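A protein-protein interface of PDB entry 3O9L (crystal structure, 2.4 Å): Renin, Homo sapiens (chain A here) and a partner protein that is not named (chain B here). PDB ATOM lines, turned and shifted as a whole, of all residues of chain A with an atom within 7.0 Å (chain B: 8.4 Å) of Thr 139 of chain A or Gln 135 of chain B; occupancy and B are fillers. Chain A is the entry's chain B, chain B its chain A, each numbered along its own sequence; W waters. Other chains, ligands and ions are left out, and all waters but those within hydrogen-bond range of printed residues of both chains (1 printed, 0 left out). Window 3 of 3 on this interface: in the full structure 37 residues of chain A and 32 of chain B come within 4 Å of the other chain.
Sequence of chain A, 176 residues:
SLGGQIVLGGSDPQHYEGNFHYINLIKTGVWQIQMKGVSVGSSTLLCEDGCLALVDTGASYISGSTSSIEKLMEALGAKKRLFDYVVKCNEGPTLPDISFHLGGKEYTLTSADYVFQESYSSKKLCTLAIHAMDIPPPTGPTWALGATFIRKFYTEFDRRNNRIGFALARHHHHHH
Of the 18 printed residues of chain B, 5 touch a printed residue of chain A. Hydrophobic or aromatic side chains of chain A within 4 Å of the printed part of chain B: Val 30 and Trp 31.
Among the printed residues, merely in contact across the chains: Gly 29 of chain A with Phe 132 of chain B, Gly 29 of chain A with Glu 134 of chain B, Gly 29 of chain A with Gln 135 of chain B, Val 30 of chain A with Phe 132 of chain B, Val 30 of chain A with Gln 135 of chain B, Trp 31 of chain A with Thr 39 of chain B, Trp 31 of chain A with Phe 132 of chain B and Thr 139 of chain A with Gln 135 of chain B.
Printed residues of chain B within 4 Å of Trp 31 of chain A: Thr 39, Met 130 and Phe 132. Pro 136 of chain A touches none of the printed residues of chain B. Pro 138 of chain A touches none of the printed residues of chain B. Of chain B, only Gln 135 comes within 4 Å of Thr 139 of chain A. No residue of chain B comes within 4 Å of Gly 140 of chain A. Ser 41 of chain B touches none of the printed residues of chain A. Printed residues of chain A within 4 Å of Met 130 of chain B: Trp 31. Printed residues of chain A within 4 Å of Glu 134 of chain B: Gly 29 (3.6 Å). Gln 135 of chain B touches just these residues of chain A: Gly 29 (3.2 Å), Val 30 (3.9 Å) and Thr 139 (3.6 Å). The nearest residue of chain A that does not touch Gln 135 of chain B is Pro 138 of chain A (6.4 Å). The nearest printed residue of chain B that does not touch Trp 31 of chain A is Gly 131 of chain B (4.2 Å).
O of Met 130 of chain B is in hydrogen-bond range of NE1 of Trp 31 of chain A (3.1 Å).
Water W1 lies within hydrogen-bond range of N of Phe 132 of chain B (2.4 Å) and O of Gly 29 of chain A (3.3 Å).
The side-chain amide oxygen (OE1) of Gln 32 of chain A sits close to the backbone carbonyl oxygen (O) of Thr 139 of chain A (3.0 Å). N of Met 130 of chain B lies within hydrogen-bond range of O of Ser 41 of chain B (3.0 Å). O of Phe 132 of chain B sits at hydrogen-bond distance from OG of Ser 42 of chain B, at 2.4 Å.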
ATOM      1  N   LYS A  27     -10.194  -2.552   3.560  1.00  0.00           N
ATOM      2  CA  LYS A  27     -11.301  -3.261   4.179  1.00  0.00           C
ATOM      3  C   LYS A  27     -10.995  -4.759   4.250  1.00  0.00           C
ATOM      4  O   LYS A  27     -10.339  -5.302   3.367  1.00  0.00           O
ATOM      5  CB  LYS A  27     -12.598  -3.014   3.389  1.00  0.00           C
ATOM      6  CG  LYS A  27     -12.535  -3.391   1.904  1.00  0.00           C
ATOM      7  CD  LYS A  27     -13.856  -4.038   1.443  1.00  0.00           C
ATOM      8  CE  LYS A  27     -14.259  -3.624   0.021  1.00  0.00           C
ATOM      9  NZ  LYS A  27     -13.139  -3.701  -0.971  1.00  0.00           N
ATOM     10  N   GLY A  29     -12.006  -8.614   3.766  1.00  0.00           N
ATOM     11  CA  GLY A  29     -12.786  -9.258   2.708  1.00  0.00           C
ATOM     12  C   GLY A  29     -11.990  -9.421   1.430  1.00  0.00           C
ATOM     13  O   GLY A  29     -12.348 -10.207   0.567  1.00  0.00           O
ATOM     14  N   VAL A  30     -10.892  -8.681   1.316  1.00  0.00           N
ATOM     15  CA  VAL A  30     -10.057  -8.673   0.110  1.00  0.00           C
ATOM     16  C   VAL A  30      -8.619  -8.273   0.483  1.00  0.00           C
ATOM     17  O   VAL A  30      -8.419  -7.406   1.340  1.00  0.00           O
ATOM     18  CB  VAL A  30     -10.687  -7.767  -1.009  1.00  0.00           C
ATOM     19  CG1 VAL A  30     -10.702  -6.289  -0.610  1.00  0.00           C
ATOM     20  CG2 VAL A  30      -9.989  -7.957  -2.342  1.00  0.00           C
ATOM     21  N   TRP A  31      -7.625  -8.929  -0.112  1.00  0.00           N
ATOM     22  CA  TRP A  31      -6.223  -8.554   0.108  1.00  0.00           C
ATOM     23  C   TRP A  31      -5.874  -7.348  -0.780  1.00  0.00           C
ATOM     24  O   TRP A  31      -5.164  -7.464  -1.787  1.00  0.00           O
ATOM     25  CB  TRP A  31      -5.270  -9.715  -0.166  1.00  0.00           C
ATOM     26  CG  TRP A  31      -5.344 -10.851   0.809  1.00  0.00           C
ATOM     27  CD1 TRP A  31      -5.841 -12.103   0.565  1.00  0.00           C
ATOM     28  CD2 TRP A  31      -4.885 -10.861   2.169  1.00  0.00           C
ATOM     29  NE1 TRP A  31      -5.721 -12.889   1.691  1.00  0.00           N
ATOM     30  CE2 TRP A  31      -5.148 -12.150   2.692  1.00  0.00           C
ATOM     31  CE3 TRP A  31      -4.298  -9.903   3.006  1.00  0.00           C
ATOM     32  CZ2 TRP A  31      -4.827 -12.507   4.016  1.00  0.00           C
ATOM     33  CZ3 TRP A  31      -3.985 -10.260   4.326  1.00  0.00           C
ATOM     34  CH2 TRP A  31      -4.252 -11.549   4.816  1.00  0.00           C
ATOM     35  N   GLN A  32      -6.392  -6.189  -0.382  1.00  0.00           N
ATOM     36  CA  GLN A  32      -6.290  -4.973  -1.170  1.00  0.00           C
ATOM     37  C   GLN A  32      -5.864  -3.796  -0.285  1.00  0.00           C
ATOM     38  O   GLN A  32      -6.419  -3.579   0.794  1.00  0.00           O
ATOM     39  CB  GLN A  32      -7.623  -4.706  -1.862  1.00  0.00           C
ATOM     40  CG  GLN A  32      -7.673  -3.479  -2.746  1.00  0.00           C
ATOM     41  CD  GLN A  32      -9.041  -3.286  -3.375  1.00  0.00           C
ATOM     42  OE1 GLN A  32      -9.157  -3.154  -4.594  1.00  0.00           O
ATOM     43  NE2 GLN A  32     -10.091  -3.290  -2.551  1.00  0.00           N
ATOM     44  N   LEU A  52      -6.014   1.985  -5.945  1.00  0.00           N
ATOM     45  CA  LEU A  52      -6.130   0.724  -5.196  1.00  0.00           C
ATOM     46  C   LEU A  52      -5.146  -0.321  -5.702  1.00  0.00           C
ATOM     47  O   LEU A  52      -4.971  -0.477  -6.912  1.00  0.00           O
ATOM     48  CB  LEU A  52      -7.555   0.179  -5.259  1.00  0.00           C
ATOM     49  CG  LEU A  52      -8.734   1.107  -4.951  1.00  0.00           C
ATOM     50  CD1 LEU A  52     -10.009   0.547  -5.568  1.00  0.00           C
ATOM     51  CD2 LEU A  52      -8.928   1.359  -3.452  1.00  0.00           C
ATOM     52  N   LEU A  54      -4.371  -4.278  -5.575  1.00  0.00           N
ATOM     53  CA  LEU A  54      -4.765  -5.635  -5.302  1.00  0.00           C
ATOM     54  C   LEU A  54      -3.517  -6.505  -5.335  1.00  0.00           C
ATOM     55  O   LEU A  54      -2.764  -6.469  -6.311  1.00  0.00           O
ATOM     56  CB  LEU A  54      -5.778  -6.067  -6.357  1.00  0.00           C
ATOM     57  CG  LEU A  54      -6.641  -7.317  -6.249  1.00  0.00           C
ATOM     58  CD1 LEU A  54      -7.150  -7.621  -4.823  1.00  0.00           C
ATOM     59  CD2 LEU A  54      -7.794  -7.121  -7.231  1.00  0.00           C
ATOM     60  N   ILE A 135     -10.912  -4.469 -14.004  1.00  0.00           N
ATOM     61  CA  ILE A 135     -11.528  -5.275 -12.963  1.00  0.00           C
ATOM     62  C   ILE A 135     -12.817  -4.567 -12.579  1.00  0.00           C
ATOM     63  O   ILE A 135     -12.850  -3.336 -12.546  1.00  0.00           O
ATOM     64  CB  ILE A 135     -10.559  -5.434 -11.749  1.00  0.00           C
ATOM     65  CG1 ILE A 135      -9.320  -6.229 -12.172  1.00  0.00           C
ATOM     66  CG2 ILE A 135     -11.233  -6.108 -10.564  1.00  0.00           C
ATOM     67  CD1 ILE A 135      -8.381  -6.570 -11.040  1.00  0.00           C
ATOM     68  N   PRO A 136     -13.899  -5.334 -12.334  1.00  0.00           N
ATOM     69  CA  PRO A 136     -15.179  -4.727 -11.996  1.00  0.00           C
ATOM     70  C   PRO A 136     -15.493  -4.720 -10.480  1.00  0.00           C
ATOM     71  O   PRO A 136     -14.943  -5.544  -9.733  1.00  0.00           O
ATOM     72  CB  PRO A 136     -16.181  -5.593 -12.773  1.00  0.00           C
ATOM     73  CG  PRO A 136     -15.503  -6.937 -12.932  1.00  0.00           C
ATOM     74  CD  PRO A 136     -14.037  -6.782 -12.565  1.00  0.00           C
ATOM     75  N   PRO A 137     -16.360  -3.775 -10.034  1.00  0.00           N
ATOM     76  CA  PRO A 137     -16.789  -3.566  -8.639  1.00  0.00           C
ATOM     77  C   PRO A 137     -17.341  -4.804  -7.916  1.00  0.00           C
ATOM     78  O   PRO A 137     -17.901  -5.691  -8.564  1.00  0.00           O
ATOM     79  CB  PRO A 137     -17.885  -2.506  -8.773  1.00  0.00           C
ATOM     80  CG  PRO A 137     -17.442  -1.685  -9.937  1.00  0.00           C
ATOM     81  CD  PRO A 137     -16.804  -2.663 -10.903  1.00  0.00           C
ATOM     82  N   PRO A 138     -17.205  -4.852  -6.571  1.00  0.00           N
ATOM     83  CA  PRO A 138     -16.598  -3.811  -5.734  1.00  0.00           C
ATOM     84  C   PRO A 138     -15.072  -3.870  -5.642  1.00  0.00           C
ATOM     85  O   PRO A 138     -14.456  -2.906  -5.178  1.00  0.00           O
ATOM     86  CB  PRO A 138     -17.225  -4.045  -4.346  1.00  0.00           C
ATOM     87  CG  PRO A 138     -18.198  -5.184  -4.508  1.00  0.00           C
ATOM     88  CD  PRO A 138     -17.794  -5.919  -5.749  1.00  0.00           C
ATOM     89  N   THR A 139     -14.467  -4.973  -6.075  1.00  0.00           N
ATOM     90  CA  THR A 139     -13.001  -5.094  -6.047  1.00  0.00           C
ATOM     91  C   THR A 139     -12.327  -4.135  -7.044  1.00  0.00           C
ATOM     92  O   THR A 139     -11.341  -3.478  -6.694  1.00  0.00           O
ATOM     93  CB  THR A 139     -12.524  -6.549  -6.287  1.00  0.00           C
ATOM     94  OG1 THR A 139     -13.421  -7.457  -5.651  1.00  0.00           O
ATOM     95  CG2 THR A 139     -11.130  -6.764  -5.713  1.00  0.00           C
ATOM     96  N   GLY A 140     -12.858  -4.055  -8.270  1.00  0.00           N
ATOM     97  CA  GLY A 140     -12.357  -3.104  -9.287  1.00  0.00           C
ATOM     98  C   GLY A 140     -13.054  -1.754  -9.241  1.00  0.00           C
ATOM     99  O   GLY A 140     -14.095  -1.639  -8.607  1.00  0.00           O
ATOM    100  N   PRO A 141     -12.484  -0.709  -9.900  1.00  0.00           N
ATOM    101  CA  PRO A 141     -11.223  -0.686 -10.645  1.00  0.00           C
ATOM    102  C   PRO A 141     -10.035  -0.592  -9.698  1.00  0.00           C
ATOM    103  O   PRO A 141     -10.124   0.070  -8.671  1.00  0.00           O
ATOM    104  CB  PRO A 141     -11.330   0.584 -11.503  1.00  0.00           C
ATOM    105  CG  PRO A 141     -12.690   1.176 -11.203  1.00  0.00           C
ATOM    106  CD  PRO A 141     -13.118   0.619  -9.903  1.00  0.00           C
ATOM    107  N   THR A 142      -8.946  -1.263 -10.058  1.00  0.00           N
ATOM    108  CA  THR A 142      -7.771  -1.414  -9.198  1.00  0.00           C
ATOM    109  C   THR A 142      -6.523  -1.714 -10.028  1.00  0.00           C
ATOM    110  O   THR A 142      -6.594  -2.088 -11.211  1.00  0.00           O
ATOM    111  CB  THR A 142      -8.009  -2.556  -8.138  1.00  0.00           C
ATOM    112  OG1 THR A 142      -6.858  -2.757  -7.307  1.00  0.00           O
ATOM    113  CG2 THR A 142      -8.344  -3.859  -8.822  1.00  0.00           C
ATOM    114  N   TRP A 143      -5.372  -1.509  -9.399  1.00  0.00           N
ATOM    115  CA  TRP A 143      -4.140  -2.103  -9.865  1.00  0.00           C
ATOM    116  C   TRP A 143      -4.118  -3.519  -9.299  1.00  0.00           C
ATOM    117  O   TRP A 143      -4.878  -3.857  -8.375  1.00  0.00           O
ATOM    118  CB  TRP A 143      -2.917  -1.285  -9.409  1.00  0.00           C
ATOM    119  CG  TRP A 143      -2.824   0.021 -10.140  1.00  0.00           C
ATOM    120  CD1 TRP A 143      -3.631   1.127  -9.967  1.00  0.00           C
ATOM    121  CD2 TRP A 143      -1.903   0.360 -11.187  1.00  0.00           C
ATOM    122  NE1 TRP A 143      -3.253   2.122 -10.833  1.00  0.00           N
ATOM    123  CE2 TRP A 143      -2.200   1.682 -11.593  1.00  0.00           C
ATOM    124  CE3 TRP A 143      -0.846  -0.319 -11.810  1.00  0.00           C
ATOM    125  CZ2 TRP A 143      -1.482   2.340 -12.597  1.00  0.00           C
ATOM    126  CZ3 TRP A 143      -0.120   0.336 -12.817  1.00  0.00           C
ATOM    127  CH2 TRP A 143      -0.448   1.651 -13.200  1.00  0.00           C
ATOM    128  N   THR B  39      -4.388 -15.553  -3.925  1.00  0.00           N
ATOM    129  CA  THR B  39      -4.937 -14.572  -2.986  1.00  0.00           C
ATOM    130  C   THR B  39      -5.991 -13.687  -3.639  1.00  0.00           C
ATOM    131  O   THR B  39      -6.689 -12.959  -2.955  1.00  0.00           O
ATOM    132  CB  THR B  39      -3.853 -13.677  -2.358  1.00  0.00           C
ATOM    133  OG1 THR B  39      -3.087 -13.070  -3.399  1.00  0.00           O
ATOM    134  CG2 THR B  39      -2.944 -14.494  -1.433  1.00  0.00           C
ATOM    135  N   GLY B  40      -6.111 -13.767  -4.959  1.00  0.00           N
ATOM    136  CA  GLY B  40      -7.165 -13.053  -5.667  1.00  0.00           C
ATOM    137  C   GLY B  40      -8.477 -13.820  -5.734  1.00  0.00           C
ATOM    138  O   GLY B  40      -9.446 -13.352  -6.339  1.00  0.00           O
ATOM    139  N   SER B  41      -8.523 -15.000  -5.122  1.00  0.00           N
ATOM    140  CA  SER B  41      -9.723 -15.828  -5.183  1.00  0.00           C
ATOM    141  C   SER B  41      -9.843 -16.705  -3.954  1.00  0.00           C
ATOM    142  O   SER B  41      -8.869 -16.884  -3.221  1.00  0.00           O
ATOM    143  CB  SER B  41      -9.749 -16.660  -6.460  1.00  0.00           C
ATOM    144  OG  SER B  41      -9.061 -17.883  -6.280  1.00  0.00           O
ATOM    145  N   SER B  42     -11.041 -17.256  -3.743  1.00  0.00           N
ATOM    146  CA  SER B  42     -11.405 -17.826  -2.456  1.00  0.00           C
ATOM    147  C   SER B  42     -11.888 -19.286  -2.441  1.00  0.00           C
ATOM    148  O   SER B  42     -12.239 -19.805  -1.386  1.00  0.00           O
ATOM    149  CB  SER B  42     -12.463 -16.936  -1.811  1.00  0.00           C
ATOM    150  OG  SER B  42     -11.871 -15.833  -1.177  1.00  0.00           O
ATOM    151  N   ASN B  43     -11.897 -19.937  -3.597  1.00  0.00           N
ATOM    152  CA  ASN B  43     -12.391 -21.293  -3.728  1.00  0.00           C
ATOM    153  C   ASN B  43     -11.283 -22.284  -4.125  1.00  0.00           C
ATOM    154  O   ASN B  43     -10.326 -21.904  -4.820  1.00  0.00           O
ATOM    155  CB  ASN B  43     -13.476 -21.319  -4.807  1.00  0.00           C
ATOM    156  CG  ASN B  43     -14.801 -20.697  -4.346  1.00  0.00           C
ATOM    157  OD1 ASN B  43     -14.988 -19.491  -4.451  1.00  0.00           O
ATOM    158  ND2 ASN B  43     -15.732 -21.536  -3.853  1.00  0.00           N
ATOM    159  N   LEU B  81     -18.746 -19.969 -12.170  1.00  0.00           N
ATOM    160  CA  LEU B  81     -17.819 -18.821 -12.215  1.00  0.00           C
ATOM    161  C   LEU B  81     -17.707 -18.293 -13.639  1.00  0.00           C
ATOM    162  O   LEU B  81     -17.514 -19.064 -14.593  1.00  0.00           O
ATOM    163  CB  LEU B  81     -16.431 -19.219 -11.706  1.00  0.00           C
ATOM    164  CG  LEU B  81     -15.374 -18.157 -11.387  1.00  0.00           C
ATOM    165  CD1 LEU B  81     -14.364 -18.766 -10.447  1.00  0.00           C
ATOM    166  CD2 LEU B  81     -14.668 -17.622 -12.636  1.00  0.00           C
ATOM    167  N   MET B 130      -6.642 -18.194  -1.670  1.00  0.00           N
ATOM    168  CA  MET B 130      -6.138 -17.782  -0.349  1.00  0.00           C
ATOM    169  C   MET B 130      -6.855 -16.537   0.154  1.00  0.00           C
ATOM    170  O   MET B 130      -6.412 -15.890   1.111  1.00  0.00           O
ATOM    171  CB  MET B 130      -4.623 -17.568  -0.348  1.00  0.00           C
ATOM    172  CG  MET B 130      -3.794 -18.817  -0.680  1.00  0.00           C
ATOM    173  SD  MET B 130      -3.993 -20.206   0.470  1.00  0.00           S
ATOM    174  CE  MET B 130      -3.050 -19.661   1.898  1.00  0.00           C
ATOM    175  N   GLY B 131      -7.980 -16.235  -0.494  1.00  0.00           N
ATOM    176  CA  GLY B 131      -8.760 -15.051  -0.197  1.00  0.00           C
ATOM    177  C   GLY B 131      -9.728 -15.274   0.945  1.00  0.00           C
ATOM    178  O   GLY B 131      -9.657 -16.281   1.658  1.00  0.00           O
ATOM    179  N   PHE B 132     -10.642 -14.323   1.091  1.00  0.00           N
ATOM    180  CA  PHE B 132     -11.610 -14.272   2.175  1.00  0.00           C
ATOM    181  C   PHE B 132     -12.950 -14.933   1.822  1.00  0.00           C
ATOM    182  O   PHE B 132     -13.264 -15.126   0.647  1.00  0.00           O
ATOM    183  CB  PHE B 132     -11.868 -12.805   2.525  1.00  0.00           C
ATOM    184  CG  PHE B 132     -10.718 -12.121   3.222  1.00  0.00           C
ATOM    185  CD1 PHE B 132      -9.744 -11.449   2.488  1.00  0.00           C
ATOM    186  CD2 PHE B 132     -10.637 -12.118   4.611  1.00  0.00           C
ATOM    187  CE1 PHE B 132      -8.695 -10.782   3.128  1.00  0.00           C
ATOM    188  CE2 PHE B 132      -9.597 -11.466   5.264  1.00  0.00           C
ATOM    189  CZ  PHE B 132      -8.611 -10.798   4.515  1.00  0.00           C
ATOM    190  N   ILE B 133     -13.739 -15.252   2.843  1.00  0.00           N
ATOM    191  CA  ILE B 133     -15.080 -15.811   2.656  1.00  0.00           C
ATOM    192  C   ILE B 133     -16.008 -14.880   1.863  1.00  0.00           C
ATOM    193  O   ILE B 133     -16.765 -15.350   1.016  1.00  0.00           O
ATOM    194  CB  ILE B 133     -15.736 -16.235   4.015  1.00  0.00           C
ATOM    195  CG1 ILE B 133     -16.937 -17.155   3.796  1.00  0.00           C
ATOM    196  CG2 ILE B 133     -16.149 -15.022   4.852  1.00  0.00           C
ATOM    197  CD1 ILE B 133     -17.353 -17.933   5.063  1.00  0.00           C
ATOM    198  N   GLU B 134     -15.945 -13.571   2.142  1.00  0.00           N
ATOM    199  CA  GLU B 134     -16.739 -12.557   1.426  1.00  0.00           C
ATOM    200  C   GLU B 134     -16.744 -12.778  -0.093  1.00  0.00           C
ATOM    201  O   GLU B 134     -17.765 -12.545  -0.754  1.00  0.00           O
ATOM    202  CB  GLU B 134     -16.221 -11.144   1.724  1.00  0.00           C
ATOM    203  CG  GLU B 134     -16.917 -10.394   2.844  1.00  0.00           C
ATOM    204  CD  GLU B 134     -16.143 -10.405   4.156  1.00  0.00           C
ATOM    205  OE1 GLU B 134     -15.296 -11.310   4.361  1.00  0.00           O
ATOM    206  OE2 GLU B 134     -16.396  -9.508   4.995  1.00  0.00           O
ATOM    207  N   GLN B 135     -15.603 -13.233  -0.625  1.00  0.00           N
ATOM    208  CA  GLN B 135     -15.416 -13.455  -2.073  1.00  0.00           C
ATOM    209  C   GLN B 135     -15.795 -14.852  -2.559  1.00  0.00           C
ATOM    210  O   GLN B 135     -16.069 -15.042  -3.761  1.00  0.00           O
ATOM    211  CB  GLN B 135     -13.957 -13.225  -2.467  1.00  0.00           C
ATOM    212  CG  GLN B 135     -13.309 -12.027  -1.830  1.00  0.00           C
ATOM    213  CD  GLN B 135     -13.752 -10.723  -2.451  1.00  0.00           C
ATOM    214  OE1 GLN B 135     -14.767 -10.131  -2.049  1.00  0.00           O
ATOM    215  NE2 GLN B 135     -12.983 -10.255  -3.430  1.00  0.00           N
ATOM    216  N   ALA B 136     -15.776 -15.817  -1.634  1.00  0.00           N
ATOM    217  CA  ALA B 136     -15.987 -17.240  -1.928  1.00  0.00           C
ATOM    218  C   ALA B 136     -17.351 -17.555  -2.555  1.00  0.00           C
ATOM    219  O   ALA B 136     -18.392 -17.126  -2.064  1.00  0.00           O
ATOM    220  CB  ALA B 136     -15.773 -18.057  -0.679  1.00  0.00           C
ATOM    221  N   ILE B 137     -17.332 -18.318  -3.638  1.00  0.00           N
ATOM    222  CA  ILE B 137     -18.548 -18.640  -4.390  1.00  0.00           C
ATOM    223  C   ILE B 137     -19.346 -19.757  -3.706  1.00  0.00           C
ATOM    224  O   ILE B 137     -18.815 -20.837  -3.416  1.00  0.00           O
ATOM    225  CB  ILE B 137     -18.229 -19.022  -5.852  1.00  0.00           C
ATOM    226  CG1 ILE B 137     -17.237 -18.021  -6.450  1.00  0.00           C
ATOM    227  CG2 ILE B 137     -19.518 -19.083  -6.679  1.00  0.00           C
ATOM    228  CD1 ILE B 137     -16.498 -18.522  -7.657  1.00  0.00           C
ATOM    229  N   GLY B 138     -20.624 -19.479  -3.457  1.00  0.00           N
ATOM    230  CA  GLY B 138     -21.488 -20.367  -2.688  1.00  0.00           C
ATOM    231  C   GLY B 138     -21.308 -20.144  -1.197  1.00  0.00           C
ATOM    232  O   GLY B 138     -21.909 -20.848  -0.379  1.00  0.00           O
ATOM    233  N   ARG B 139     -20.470 -19.166  -0.850  1.00  0.00           N
ATOM    234  CA  ARG B 139     -20.081 -18.887   0.540  1.00  0.00           C
ATOM    235  C   ARG B 139     -19.500 -20.128   1.252  1.00  0.00           C
ATOM    236  O   ARG B 139     -19.570 -20.263   2.477  1.00  0.00           O
ATOM    237  CB  ARG B 139     -21.230 -18.225   1.330  1.00  0.00           C
ATOM    238  CG  ARG B 139     -20.763 -17.487   2.585  1.00  0.00           C
ATOM    239  CD  ARG B 139     -21.695 -16.343   2.968  1.00  0.00           C
ATOM    240  NE  ARG B 139     -21.248 -15.674   4.191  1.00  0.00           N
ATOM    241  CZ  ARG B 139     -20.432 -14.624   4.219  1.00  0.00           C
ATOM    242  NH1 ARG B 139     -19.961 -14.112   3.087  1.00  0.00           N
ATOM    243  NH2 ARG B 139     -20.079 -14.087   5.384  1.00  0.00           N
ATOM    244  N   VAL B 140     -18.910 -21.016   0.454  1.00  0.00           N
ATOM    245  CA  VAL B 140     -18.065 -22.104   0.941  1.00  0.00           C
ATOM    246  C   VAL B 140     -16.843 -21.553   1.678  1.00  0.00           C
ATOM    247  O   VAL B 140     -16.239 -20.566   1.248  1.00  0.00           O
ATOM    248  CB  VAL B 140     -17.559 -22.970  -0.239  1.00  0.00           C
ATOM    249  CG1 VAL B 140     -16.623 -24.055   0.246  1.00  0.00           C
ATOM    250  CG2 VAL B 140     -18.727 -23.552  -1.029  1.00  0.00           C
ATOM    251  N   PRO B 142     -13.161 -21.000   2.865  1.00  0.00           N
ATOM    252  CA  PRO B 142     -11.825 -21.120   2.275  1.00  0.00           C
ATOM    253  C   PRO B 142     -10.858 -21.960   3.110  1.00  0.00           C
ATOM    254  O   PRO B 142     -11.064 -22.149   4.308  1.00  0.00           O
ATOM    255  CB  PRO B 142     -11.352 -19.673   2.171  1.00  0.00           C
ATOM    256  CG  PRO B 142     -12.596 -18.874   2.169  1.00  0.00           C
ATOM    257  CD  PRO B 142     -13.511 -19.595   3.107  1.00  0.00           C
HETATM  258  O   HOH W   1     -10.444 -12.593  -0.565  1.00  0.00           O
